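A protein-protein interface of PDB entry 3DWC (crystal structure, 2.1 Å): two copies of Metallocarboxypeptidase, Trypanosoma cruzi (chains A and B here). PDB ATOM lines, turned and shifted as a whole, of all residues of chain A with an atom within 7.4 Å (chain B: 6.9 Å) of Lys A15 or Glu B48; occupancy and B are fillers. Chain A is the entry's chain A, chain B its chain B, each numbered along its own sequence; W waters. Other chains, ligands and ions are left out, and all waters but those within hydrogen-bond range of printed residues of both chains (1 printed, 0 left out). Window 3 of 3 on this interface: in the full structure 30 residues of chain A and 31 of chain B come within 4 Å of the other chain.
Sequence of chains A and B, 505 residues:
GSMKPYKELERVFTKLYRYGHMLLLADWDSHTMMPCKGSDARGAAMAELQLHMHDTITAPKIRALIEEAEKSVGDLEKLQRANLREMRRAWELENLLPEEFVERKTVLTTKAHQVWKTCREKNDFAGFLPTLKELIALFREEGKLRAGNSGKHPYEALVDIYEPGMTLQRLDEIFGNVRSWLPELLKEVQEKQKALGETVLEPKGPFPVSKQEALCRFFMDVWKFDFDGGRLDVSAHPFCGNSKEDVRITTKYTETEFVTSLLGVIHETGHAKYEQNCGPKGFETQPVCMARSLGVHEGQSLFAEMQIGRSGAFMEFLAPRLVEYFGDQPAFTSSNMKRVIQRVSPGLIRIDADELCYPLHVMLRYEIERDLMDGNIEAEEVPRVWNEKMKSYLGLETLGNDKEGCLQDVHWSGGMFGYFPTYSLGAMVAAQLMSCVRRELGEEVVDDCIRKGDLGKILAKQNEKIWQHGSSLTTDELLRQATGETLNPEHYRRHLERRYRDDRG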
ATOM      1  N   GLU A   8      -1.232  34.119  35.244  1.00  0.00           N
ATOM      2  CA  GLU A   8      -1.033  33.446  33.967  1.00  0.00           C
ATOM      3  C   GLU A   8      -1.578  32.008  33.949  1.00  0.00           C
ATOM      4  O   GLU A   8      -2.081  31.569  32.931  1.00  0.00           O
ATOM      5  CB  GLU A   8       0.440  33.435  33.590  1.00  0.00           C
ATOM      6  CG  GLU A   8       0.742  32.723  32.267  1.00  0.00           C
ATOM      7  CD  GLU A   8       0.214  33.438  31.005  1.00  0.00           C
ATOM      8  OE1 GLU A   8       0.073  32.738  29.965  1.00  0.00           O
ATOM      9  OE2 GLU A   8      -0.067  34.673  31.042  1.00  0.00           O
ATOM     10  N   LEU A   9      -1.460  31.263  35.052  1.00  0.00           N
ATOM     11  CA  LEU A   9      -2.094  29.948  35.148  1.00  0.00           C
ATOM     12  C   LEU A   9      -3.606  30.045  35.040  1.00  0.00           C
ATOM     13  O   LEU A   9      -4.228  29.244  34.354  1.00  0.00           O
ATOM     14  CB  LEU A   9      -1.737  29.214  36.433  1.00  0.00           C
ATOM     15  CG  LEU A   9      -0.330  28.660  36.505  1.00  0.00           C
ATOM     16  CD1 LEU A   9       0.081  28.396  37.959  1.00  0.00           C
ATOM     17  CD2 LEU A   9      -0.170  27.407  35.572  1.00  0.00           C
ATOM     18  N   GLU A  10      -4.186  31.023  35.702  1.00  0.00           N
ATOM     19  CA  GLU A  10      -5.637  31.284  35.611  1.00  0.00           C
ATOM     20  C   GLU A  10      -6.071  31.448  34.157  1.00  0.00           C
ATOM     21  O   GLU A  10      -7.104  30.889  33.744  1.00  0.00           O
ATOM     22  CB  GLU A  10      -6.011  32.560  36.411  1.00  0.00           C
ATOM     23  CG  GLU A  10      -6.176  32.340  37.915  1.00  0.00           C
ATOM     24  CD  GLU A  10      -6.993  33.450  38.594  1.00  0.00           C
ATOM     25  OE1 GLU A  10      -7.044  34.569  38.056  1.00  0.00           O
ATOM     26  OE2 GLU A  10      -7.592  33.213  39.674  1.00  0.00           O
ATOM     27  N   ARG A  11      -5.294  32.229  33.404  1.00  0.00           N
ATOM     28  CA  ARG A  11      -5.528  32.453  31.958  1.00  0.00           C
ATOM     29  C   ARG A  11      -5.418  31.119  31.181  1.00  0.00           C
ATOM     30  O   ARG A  11      -6.292  30.761  30.366  1.00  0.00           O
ATOM     31  CB  ARG A  11      -4.555  33.552  31.452  1.00  0.00           C
ATOM     32  CG  ARG A  11      -4.869  34.135  30.041  1.00  0.00           C
ATOM     33  CD  ARG A  11      -3.740  35.060  29.329  1.00  0.00           C
ATOM     34  NE  ARG A  11      -2.551  34.305  28.849  1.00  0.00           N
ATOM     35  CZ  ARG A  11      -2.548  33.372  27.874  1.00  0.00           C
ATOM     36  NH1 ARG A  11      -1.413  32.745  27.546  1.00  0.00           N
ATOM     37  NH2 ARG A  11      -3.665  33.024  27.227  1.00  0.00           N
ATOM     38  N   VAL A  12      -4.390  30.332  31.475  1.00  0.00           N
ATOM     39  CA  VAL A  12      -4.288  28.991  30.875  1.00  0.00           C
ATOM     40  C   VAL A  12      -5.481  28.069  31.186  1.00  0.00           C
ATOM     41  O   VAL A  12      -6.039  27.457  30.270  1.00  0.00           O
ATOM     42  CB  VAL A  12      -2.987  28.248  31.195  1.00  0.00           C
ATOM     43  CG1 VAL A  12      -2.998  26.848  30.476  1.00  0.00           C
ATOM     44  CG2 VAL A  12      -1.797  29.035  30.710  1.00  0.00           C
ATOM     45  N   PHE A  13      -5.901  27.995  32.449  1.00  0.00           N
ATOM     46  CA  PHE A  13      -7.010  27.132  32.785  1.00  0.00           C
ATOM     47  C   PHE A  13      -8.352  27.652  32.205  1.00  0.00           C
ATOM     48  O   PHE A  13      -9.205  26.853  31.885  1.00  0.00           O
ATOM     49  CB  PHE A  13      -7.082  26.867  34.264  1.00  0.00           C
ATOM     50  CG  PHE A  13      -6.182  25.782  34.717  1.00  0.00           C
ATOM     51  CD1 PHE A  13      -4.844  26.032  34.947  1.00  0.00           C
ATOM     52  CD2 PHE A  13      -6.637  24.504  34.874  1.00  0.00           C
ATOM     53  CE1 PHE A  13      -3.982  25.023  35.354  1.00  0.00           C
ATOM     54  CE2 PHE A  13      -5.747  23.501  35.278  1.00  0.00           C
ATOM     55  CZ  PHE A  13      -4.440  23.788  35.512  1.00  0.00           C
ATOM     56  N   THR A  14      -8.542  28.957  32.044  1.00  0.00           N
ATOM     57  CA  THR A  14      -9.720  29.428  31.317  1.00  0.00           C
ATOM     58  C   THR A  14      -9.751  28.890  29.845  1.00  0.00           C
ATOM     59  O   THR A  14     -10.779  28.419  29.367  1.00  0.00           O
ATOM     60  CB  THR A  14      -9.819  30.941  31.383  1.00  0.00           C
ATOM     61  OG1 THR A  14      -9.955  31.364  32.760  1.00  0.00           O
ATOM     62  CG2 THR A  14     -11.003  31.479  30.549  1.00  0.00           C
ATOM     63  N   LYS A  15      -8.611  28.962  29.175  1.00  0.00           N
ATOM     64  CA  LYS A  15      -8.413  28.437  27.842  1.00  0.00           C
ATOM     65  C   LYS A  15      -8.850  26.970  27.794  1.00  0.00           C
ATOM     66  O   LYS A  15      -9.737  26.594  27.036  1.00  0.00           O
ATOM     67  CB  LYS A  15      -6.948  28.636  27.459  1.00  0.00           C
ATOM     68  CG  LYS A  15      -6.594  28.279  26.059  1.00  0.00           C
ATOM     69  CD  LYS A  15      -5.214  28.891  25.658  1.00  0.00           C
ATOM     70  CE  LYS A  15      -4.086  28.164  26.361  1.00  0.00           C
ATOM     71  NZ  LYS A  15      -2.767  28.351  25.615  1.00  0.00           N
ATOM     72  N   LEU A  16      -8.290  26.175  28.678  1.00  0.00           N
ATOM     73  CA  LEU A  16      -8.644  24.775  28.833  1.00  0.00           C
ATOM     74  C   LEU A  16     -10.117  24.604  29.127  1.00  0.00           C
ATOM     75  O   LEU A  16     -10.703  23.684  28.632  1.00  0.00           O
ATOM     76  CB  LEU A  16      -7.795  24.138  29.923  1.00  0.00           C
ATOM     77  CG  LEU A  16      -6.299  23.946  29.602  1.00  0.00           C
ATOM     78  CD1 LEU A  16      -5.571  23.352  30.809  1.00  0.00           C
ATOM     79  CD2 LEU A  16      -6.086  23.071  28.356  1.00  0.00           C
ATOM     80  N   TYR A  17     -10.720  25.509  29.903  1.00  0.00           N
ATOM     81  CA  TYR A  17     -12.150  25.418  30.227  1.00  0.00           C
ATOM     82  C   TYR A  17     -12.953  25.608  28.901  1.00  0.00           C
ATOM     83  O   TYR A  17     -13.913  24.883  28.636  1.00  0.00           O
ATOM     84  CB  TYR A  17     -12.507  26.476  31.289  1.00  0.00           C
ATOM     85  CG  TYR A  17     -13.955  26.495  31.751  1.00  0.00           C
ATOM     86  CD1 TYR A  17     -14.424  25.548  32.676  1.00  0.00           C
ATOM     87  CD2 TYR A  17     -14.845  27.392  31.240  1.00  0.00           C
ATOM     88  CE1 TYR A  17     -15.714  25.539  33.070  1.00  0.00           C
ATOM     89  CE2 TYR A  17     -16.154  27.427  31.670  1.00  0.00           C
ATOM     90  CZ  TYR A  17     -16.579  26.485  32.574  1.00  0.00           C
ATOM     91  OH  TYR A  17     -17.881  26.486  33.006  1.00  0.00           O
ATOM     92  N   ARG A  18     -12.528  26.573  28.080  1.00  0.00           N
ATOM     93  CA  ARG A  18     -13.171  26.868  26.810  1.00  0.00           C
ATOM     94  C   ARG A  18     -13.107  25.687  25.869  1.00  0.00           C
ATOM     95  O   ARG A  18     -14.126  25.312  25.294  1.00  0.00           O
ATOM     96  CB  ARG A  18     -12.508  28.087  26.142  1.00  0.00           C
ATOM     97  CG  ARG A  18     -12.662  29.425  26.922  1.00  0.00           C
ATOM     98  CD  ARG A  18     -14.001  29.618  27.568  1.00  0.00           C
ATOM     99  NE  ARG A  18     -14.038  30.910  28.277  1.00  0.00           N
ATOM    100  CZ  ARG A  18     -15.020  31.270  29.071  1.00  0.00           C
ATOM    101  NH1 ARG A  18     -16.052  30.482  29.250  1.00  0.00           N
ATOM    102  NH2 ARG A  18     -14.977  32.438  29.710  1.00  0.00           N
ATOM    103  N   TYR A  19     -11.925  25.084  25.748  1.00  0.00           N
ATOM    104  CA  TYR A  19     -11.756  23.829  25.015  1.00  0.00           C
ATOM    105  C   TYR A  19     -12.658  22.701  25.568  1.00  0.00           C
ATOM    106  O   TYR A  19     -13.281  21.944  24.786  1.00  0.00           O
ATOM    107  CB  TYR A  19     -10.278  23.368  24.939  1.00  0.00           C
ATOM    108  CG  TYR A  19      -9.235  24.341  24.326  1.00  0.00           C
ATOM    109  CD1 TYR A  19      -9.535  25.157  23.268  1.00  0.00           C
ATOM    110  CD2 TYR A  19      -7.923  24.400  24.822  1.00  0.00           C
ATOM    111  CE1 TYR A  19      -8.600  26.041  22.727  1.00  0.00           C
ATOM    112  CE2 TYR A  19      -6.958  25.261  24.268  1.00  0.00           C
ATOM    113  CZ  TYR A  19      -7.316  26.107  23.217  1.00  0.00           C
ATOM    114  OH  TYR A  19      -6.385  27.017  22.618  1.00  0.00           O
ATOM    115  N   GLY A  20     -12.703  22.532  26.894  1.00  0.00           N
ATOM    116  CA  GLY A  20     -13.506  21.441  27.499  1.00  0.00           C
ATOM    117  C   GLY A  20     -14.993  21.624  27.213  1.00  0.00           C
ATOM    118  O   GLY A  20     -15.733  20.652  27.069  1.00  0.00           O
ATOM    119  N   HIS A  21     -15.430  22.866  27.100  1.00  0.00           N
ATOM    120  CA  HIS A  21     -16.807  23.165  26.702  1.00  0.00           C
ATOM    121  C   HIS A  21     -17.176  22.490  25.372  1.00  0.00           C
ATOM    122  O   HIS A  21     -18.235  21.874  25.236  1.00  0.00           O
ATOM    123  CB  HIS A  21     -17.008  24.674  26.623  1.00  0.00           C
ATOM    124  CG  HIS A  21     -18.328  25.090  26.042  1.00  0.00           C
ATOM    125  ND1 HIS A  21     -19.313  25.686  26.796  1.00  0.00           N
ATOM    126  CD2 HIS A  21     -18.808  25.032  24.773  1.00  0.00           C
ATOM    127  CE1 HIS A  21     -20.344  25.968  26.021  1.00  0.00           C
ATOM    128  NE2 HIS A  21     -20.075  25.560  24.798  1.00  0.00           N
ATOM    129  N   MET A  22     -16.266  22.594  24.416  1.00  0.00           N
ATOM    130  CA  MET A  22     -16.482  22.043  23.102  1.00  0.00           C
ATOM    131  C   MET A  22     -16.525  20.527  23.177  1.00  0.00           C
ATOM    132  O   MET A  22     -17.379  19.892  22.577  1.00  0.00           O
ATOM    133  CB  MET A  22     -15.374  22.508  22.155  1.00  0.00           C
ATOM    134  CG  MET A  22     -15.420  24.011  21.877  1.00  0.00           C
ATOM    135  SD  MET A  22     -16.903  24.327  20.877  1.00  0.00           S
ATOM    136  CE  MET A  22     -16.815  26.041  20.618  1.00  0.00           C
ATOM    137  N   HIS A  52      -4.872  18.635  21.777  1.00  0.00           N
ATOM    138  CA  HIS A  52      -4.474  20.005  22.010  1.00  0.00           C
ATOM    139  C   HIS A  52      -4.562  20.398  23.510  1.00  0.00           C
ATOM    140  O   HIS A  52      -3.661  21.079  24.046  1.00  0.00           O
ATOM    141  CB  HIS A  52      -5.300  20.953  21.134  1.00  0.00           C
ATOM    142  CG  HIS A  52      -5.001  22.383  21.370  1.00  0.00           C
ATOM    143  ND1 HIS A  52      -3.736  22.911  21.205  1.00  0.00           N
ATOM    144  CD2 HIS A  52      -5.777  23.387  21.833  1.00  0.00           C
ATOM    145  CE1 HIS A  52      -3.752  24.184  21.546  1.00  0.00           C
ATOM    146  NE2 HIS A  52      -4.983  24.507  21.911  1.00  0.00           N
ATOM    147  N   MET A  53      -5.642  19.982  24.177  1.00  0.00           N
ATOM    148  CA  MET A  53      -5.785  20.146  25.612  1.00  0.00           C
ATOM    149  C   MET A  53      -4.660  19.479  26.402  1.00  0.00           C
ATOM    150  O   MET A  53      -4.103  20.085  27.310  1.00  0.00           O
ATOM    151  CB  MET A  53      -7.125  19.605  26.100  1.00  0.00           C
ATOM    152  CG  MET A  53      -8.284  20.449  25.678  1.00  0.00           C
ATOM    153  SD  MET A  53      -9.851  19.739  26.133  1.00  0.00           S
ATOM    154  CE  MET A  53      -9.788  19.902  27.915  1.00  0.00           C
ATOM    155  N   THR A  56      -1.411  21.339  25.845  1.00  0.00           N
ATOM    156  CA  THR A  56      -1.499  22.618  26.541  1.00  0.00           C
ATOM    157  C   THR A  56      -1.153  22.468  28.017  1.00  0.00           C
ATOM    158  O   THR A  56      -0.297  23.211  28.546  1.00  0.00           O
ATOM    159  CB  THR A  56      -2.868  23.283  26.316  1.00  0.00           C
ATOM    160  OG1 THR A  56      -2.984  23.568  24.933  1.00  0.00           O
ATOM    161  CG2 THR A  56      -3.055  24.620  27.120  1.00  0.00           C
ATOM    162  N   LYS A  61       6.239  24.680  30.264  1.00  0.00           N
ATOM    163  CA  LYS A  61       5.748  25.982  30.725  1.00  0.00           C
ATOM    164  C   LYS A  61       4.817  25.886  31.948  1.00  0.00           C
ATOM    165  O   LYS A  61       4.947  26.648  32.910  1.00  0.00           O
ATOM    166  CB  LYS A  61       5.006  26.646  29.554  1.00  0.00           C
ATOM    167  CG  LYS A  61       3.988  27.714  29.901  1.00  0.00           C
ATOM    168  CD  LYS A  61       3.238  28.253  28.607  1.00  0.00           C
ATOM    169  CE  LYS A  61       2.317  29.502  28.879  1.00  0.00           C
ATOM    170  NZ  LYS A  61       1.338  29.836  27.727  1.00  0.00           N
ATOM    171  N   ILE A  62       3.878  24.944  31.917  1.00  0.00           N
ATOM    172  CA  ILE A  62       2.917  24.814  33.011  1.00  0.00           C
ATOM    173  C   ILE A  62       3.594  24.426  34.348  1.00  0.00           C
ATOM    174  O   ILE A  62       3.316  25.007  35.410  1.00  0.00           O
ATOM    175  CB  ILE A  62       1.772  23.849  32.642  1.00  0.00           C
ATOM    176  CG1 ILE A  62       1.134  24.287  31.327  1.00  0.00           C
ATOM    177  CG2 ILE A  62       0.738  23.789  33.769  1.00  0.00           C
ATOM    178  CD1 ILE A  62       0.837  25.820  31.210  1.00  0.00           C
ATOM    179  N   THR A 285     -14.470  29.567  35.611  1.00  0.00           N
ATOM    180  CA  THR A 285     -13.640  28.886  34.558  1.00  0.00           C
ATOM    181  C   THR A 285     -12.393  28.211  35.129  1.00  0.00           C
ATOM    182  O   THR A 285     -11.548  27.745  34.382  1.00  0.00           O
ATOM    183  CB  THR A 285     -13.173  29.901  33.514  1.00  0.00           C
ATOM    184  OG1 THR A 285     -12.262  30.820  34.126  1.00  0.00           O
ATOM    185  CG2 THR A 285     -14.383  30.679  32.910  1.00  0.00           C
ATOM    186  N   GLN A 286     -12.323  28.098  36.459  1.00  0.00           N
ATOM    187  CA  GLN A 286     -11.153  27.579  37.190  1.00  0.00           C
ATOM    188  C   GLN A 286     -11.369  26.244  37.865  1.00  0.00           C
ATOM    189  O   GLN A 286     -12.504  25.862  38.211  1.00  0.00           O
ATOM    190  CB  GLN A 286     -10.758  28.583  38.292  1.00  0.00           C
ATOM    191  CG  GLN A 286     -10.336  29.927  37.802  1.00  0.00           C
ATOM    192  CD  GLN A 286      -9.107  29.850  36.870  1.00  0.00           C
ATOM    193  OE1 GLN A 286      -8.041  29.316  37.247  1.00  0.00           O
ATOM    194  NE2 GLN A 286      -9.234  30.426  35.672  1.00  0.00           N
ATOM    195  N   LEU B  23     -16.605  23.875  15.930  1.00  0.00           N
ATOM    196  CA  LEU B  23     -17.229  25.176  15.734  1.00  0.00           C
ATOM    197  C   LEU B  23     -18.595  25.080  15.058  1.00  0.00           C
ATOM    198  O   LEU B  23     -19.547  25.724  15.454  1.00  0.00           O
ATOM    199  CB  LEU B  23     -16.332  26.054  14.846  1.00  0.00           C
ATOM    200  CG  LEU B  23     -15.229  26.846  15.523  1.00  0.00           C
ATOM    201  CD1 LEU B  23     -14.608  27.807  14.498  1.00  0.00           C
ATOM    202  CD2 LEU B  23     -15.800  27.590  16.708  1.00  0.00           C
ATOM    203  N   GLY B  43     -20.296  31.394  23.561  1.00  0.00           N
ATOM    204  CA  GLY B  43     -19.651  32.408  22.698  1.00  0.00           C
ATOM    205  C   GLY B  43     -18.191  32.512  23.068  1.00  0.00           C
ATOM    206  O   GLY B  43     -17.349  32.516  22.183  1.00  0.00           O
ATOM    207  N   ALA B  44     -17.906  32.468  24.364  1.00  0.00           N
ATOM    208  CA  ALA B  44     -16.516  32.426  24.888  1.00  0.00           C
ATOM    209  C   ALA B  44     -15.728  31.209  24.339  1.00  0.00           C
ATOM    210  O   ALA B  44     -14.550  31.304  23.917  1.00  0.00           O
ATOM    211  CB  ALA B  44     -16.544  32.463  26.388  1.00  0.00           C
ATOM    212  N   ALA B  45     -16.407  30.076  24.232  1.00  0.00           N
ATOM    213  CA  ALA B  45     -15.768  28.843  23.782  1.00  0.00           C
ATOM    214  C   ALA B  45     -15.506  28.873  22.286  1.00  0.00           C
ATOM    215  O   ALA B  45     -14.429  28.503  21.828  1.00  0.00           O
ATOM    216  CB  ALA B  45     -16.623  27.651  24.169  1.00  0.00           C
ATOM    217  N   MET B  46     -16.503  29.290  21.516  1.00  0.00           N
ATOM    218  CA  MET B  46     -16.343  29.502  20.094  1.00  0.00           C
ATOM    219  C   MET B  46     -15.218  30.491  19.758  1.00  0.00           C
ATOM    220  O   MET B  46     -14.422  30.228  18.887  1.00  0.00           O
ATOM    221  CB  MET B  46     -17.688  29.973  19.537  1.00  0.00           C
ATOM    222  CG  MET B  46     -18.675  28.801  19.501  1.00  0.00           C
ATOM    223  SD  MET B  46     -20.288  29.214  18.865  1.00  0.00           S
ATOM    224  CE  MET B  46     -19.973  29.444  17.118  1.00  0.00           C
ATOM    225  N   ALA B  47     -15.095  31.578  20.518  1.00  0.00           N
ATOM    226  CA  ALA B  47     -14.064  32.583  20.307  1.00  0.00           C
ATOM    227  C   ALA B  47     -12.685  32.036  20.531  1.00  0.00           C
ATOM    228  O   ALA B  47     -11.754  32.394  19.806  1.00  0.00           O
ATOM    229  CB  ALA B  47     -14.254  33.813  21.266  1.00  0.00           C
ATOM    230  N   GLU B  48     -12.523  31.268  21.605  1.00  0.00           N
ATOM    231  CA  GLU B  48     -11.237  30.691  21.923  1.00  0.00           C
ATOM    232  C   GLU B  48     -10.812  29.705  20.836  1.00  0.00           C
ATOM    233  O   GLU B  48      -9.676  29.701  20.387  1.00  0.00           O
ATOM    234  CB  GLU B  48     -11.255  29.996  23.295  1.00  0.00           C
ATOM    235  CG  GLU B  48      -9.871  29.556  23.750  1.00  0.00           C
ATOM    236  CD  GLU B  48      -8.896  30.718  23.939  1.00  0.00           C
ATOM    237  OE1 GLU B  48      -7.756  30.633  23.468  1.00  0.00           O
ATOM    238  OE2 GLU B  48      -9.269  31.730  24.500  1.00  0.00           O
ATOM    239  N   LEU B  49     -11.729  28.890  20.385  1.00  0.00           N
ATOM    240  CA  LEU B  49     -11.403  27.912  19.311  1.00  0.00           C
ATOM    241  C   LEU B  49     -11.123  28.604  17.951  1.00  0.00           C
ATOM    242  O   LEU B  49     -10.196  28.224  17.237  1.00  0.00           O
ATOM    243  CB  LEU B  49     -12.516  26.878  19.142  1.00  0.00           C
ATOM    244  CG  LEU B  49     -12.137  25.390  18.895  1.00  0.00           C
ATOM    245  CD1 LEU B  49     -13.288  24.643  18.281  1.00  0.00           C
ATOM    246  CD2 LEU B  49     -10.889  25.199  18.056  1.00  0.00           C
ATOM    247  N   GLN B  50     -11.917  29.615  17.607  1.00  0.00           N
ATOM    248  CA  GLN B  50     -11.662  30.462  16.434  1.00  0.00           C
ATOM    249  C   GLN B  50     -10.253  31.021  16.518  1.00  0.00           C
ATOM    250  O   GLN B  50      -9.545  31.000  15.531  1.00  0.00           O
ATOM    251  CB  GLN B  50     -12.680  31.624  16.299  1.00  0.00           C
ATOM    252  CG  GLN B  50     -14.132  31.197  15.965  1.00  0.00           C
ATOM    253  CD  GLN B  50     -15.258  32.282  16.208  1.00  0.00           C
ATOM    254  OE1 GLN B  50     -15.013  33.392  16.664  1.00  0.00           O
ATOM    255  NE2 GLN B  50     -16.500  31.906  15.904  1.00  0.00           N
ATOM    256  N   LEU B  51      -9.850  31.511  17.694  1.00  0.00           N
ATOM    257  CA  LEU B  51      -8.488  32.036  17.908  1.00  0.00           C
ATOM    258  C   LEU B  51      -7.407  31.008  17.524  1.00  0.00           C
ATOM    259  O   LEU B  51      -6.465  31.307  16.770  1.00  0.00           O
ATOM    260  CB  LEU B  51      -8.314  32.476  19.352  1.00  0.00           C
ATOM    261  CG  LEU B  51      -7.229  33.467  19.748  1.00  0.00           C
ATOM    262  CD1 LEU B  51      -7.195  33.621  21.246  1.00  0.00           C
ATOM    263  CD2 LEU B  51      -5.889  33.016  19.286  1.00  0.00           C
ATOM    264  N   HIS B  52      -7.566  29.784  18.010  1.00  0.00           N
ATOM    265  CA  HIS B  52      -6.580  28.735  17.782  1.00  0.00           C
ATOM    266  C   HIS B  52      -6.501  28.435  16.285  1.00  0.00           C
ATOM    267  O   HIS B  52      -5.422  28.376  15.705  1.00  0.00           O
ATOM    268  CB  HIS B  52      -6.914  27.489  18.605  1.00  0.00           C
ATOM    269  CG  HIS B  52      -5.898  26.392  18.488  1.00  0.00           C
ATOM    270  ND1 HIS B  52      -4.573  26.573  18.794  1.00  0.00           N
ATOM    271  CD2 HIS B  52      -6.014  25.115  18.050  1.00  0.00           C
ATOM    272  CE1 HIS B  52      -3.913  25.452  18.560  1.00  0.00           C
ATOM    273  NE2 HIS B  52      -4.767  24.551  18.107  1.00  0.00           N
ATOM    274  N   MET B  53      -7.653  28.299  15.639  1.00  0.00           N
ATOM    275  CA  MET B  53      -7.669  28.082  14.194  1.00  0.00           C
ATOM    276  C   MET B  53      -6.943  29.215  13.489  1.00  0.00           C
ATOM    277  O   MET B  53      -6.147  28.975  12.590  1.00  0.00           O
ATOM    278  CB  MET B  53      -9.082  27.967  13.686  1.00  0.00           C
ATOM    279  CG  MET B  53      -9.806  26.806  14.281  1.00  0.00           C
ATOM    280  SD  MET B  53     -11.468  26.643  13.667  1.00  0.00           S
ATOM    281  CE  MET B  53     -11.175  26.254  11.938  1.00  0.00           C
ATOM    282  N   ASP B  55      -4.471  31.251  14.724  1.00  0.00           N
ATOM    283  CA  ASP B  55      -3.044  31.124  15.003  1.00  0.00           C
ATOM    284  C   ASP B  55      -2.405  29.977  14.224  1.00  0.00           C
ATOM    285  O   ASP B  55      -1.269  30.084  13.783  1.00  0.00           O
ATOM    286  CB  ASP B  55      -2.804  30.876  16.493  1.00  0.00           C
ATOM    287  CG  ASP B  55      -3.144  32.066  17.352  1.00  0.00           C
ATOM    288  OD1 ASP B  55      -3.361  33.170  16.817  1.00  0.00           O
ATOM    289  OD2 ASP B  55      -3.218  31.896  18.574  1.00  0.00           O
HETATM  290  O   HOH W   1      -6.800  29.186  21.667  1.00  0.00           O
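The side-chain hydroxyl of Tyr A19 lies within hydrogen-bond range of a ring nitrogen (NE2) of His A52. O of His A52 lies within hydrogen-bond range of OG1 of Thr A56 (2.7 Å).
OE1 of Glu B48 touches CG of Lys A15, at 3.7 Å. Arg A18 touches Ala B44 (CZ to CB, 3.3 Å). Arg A18 touches Ala B45. Arg A18 touches Glu B48 (CB to CB, 3.6 Å). Tyr A19 touches Glu B48 (CE1 to CG, 3.9 Å). Ala B45 touches His A21. Met A22 touches Ala B45. N of Met B46 touches CE of Met A22, at 3.4 Å. His A52 touches His B52 (CE1 to CE1, 3.2 Å).
Of chain B, only Glu B48 (3.7 Å) comes within 4 Å of Lys A15. Printed residues of chain A within 4 Å of Met B46: Met A22 (3.4 Å). No residue of chain A comes within 4 Å of Ala B47. Glu B48 touches three residues of chain A. Printed residues of chain A within 4 Å of His B52: His A52 (3.2 Å). The nearest residue of chain B that does not touch Lys A15 is Leu B51 (6.8 Å). The nearest residue of chain A that does not touch Glu B48 is Thr A14 (5.8 Å).
Hydrophobic or aromatic side chains of chain A that line the printed part of chain B: Tyr A19, His A21, Met A22 and His A52. Of the 13 printed residues of chain B, 5 touch a printed residue of chain A. Hydrophobic or aromatic side chains of chain B within 4 Å of the printed part of chain A: Ala B44, Ala B45, Met B46 and His B52. Among the printed residues, no Asp or Glu carboxylate lies within 4 Å of a Lys or Arg side-chain nitrogen of the other chain.
His A52 touches its own counterpart, His B52. 2 positions are printed for both chains. Of the 9 pairs that touch across the chains among the printed residues, 1 has its exchanged pair printed and touching as well.
Water W1 bridges the side-chain hydroxyl (OH) of Tyr A19 (2.4 Å) and the side-chain carboxylate (OE1) of Glu B48 (2.5 Å).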
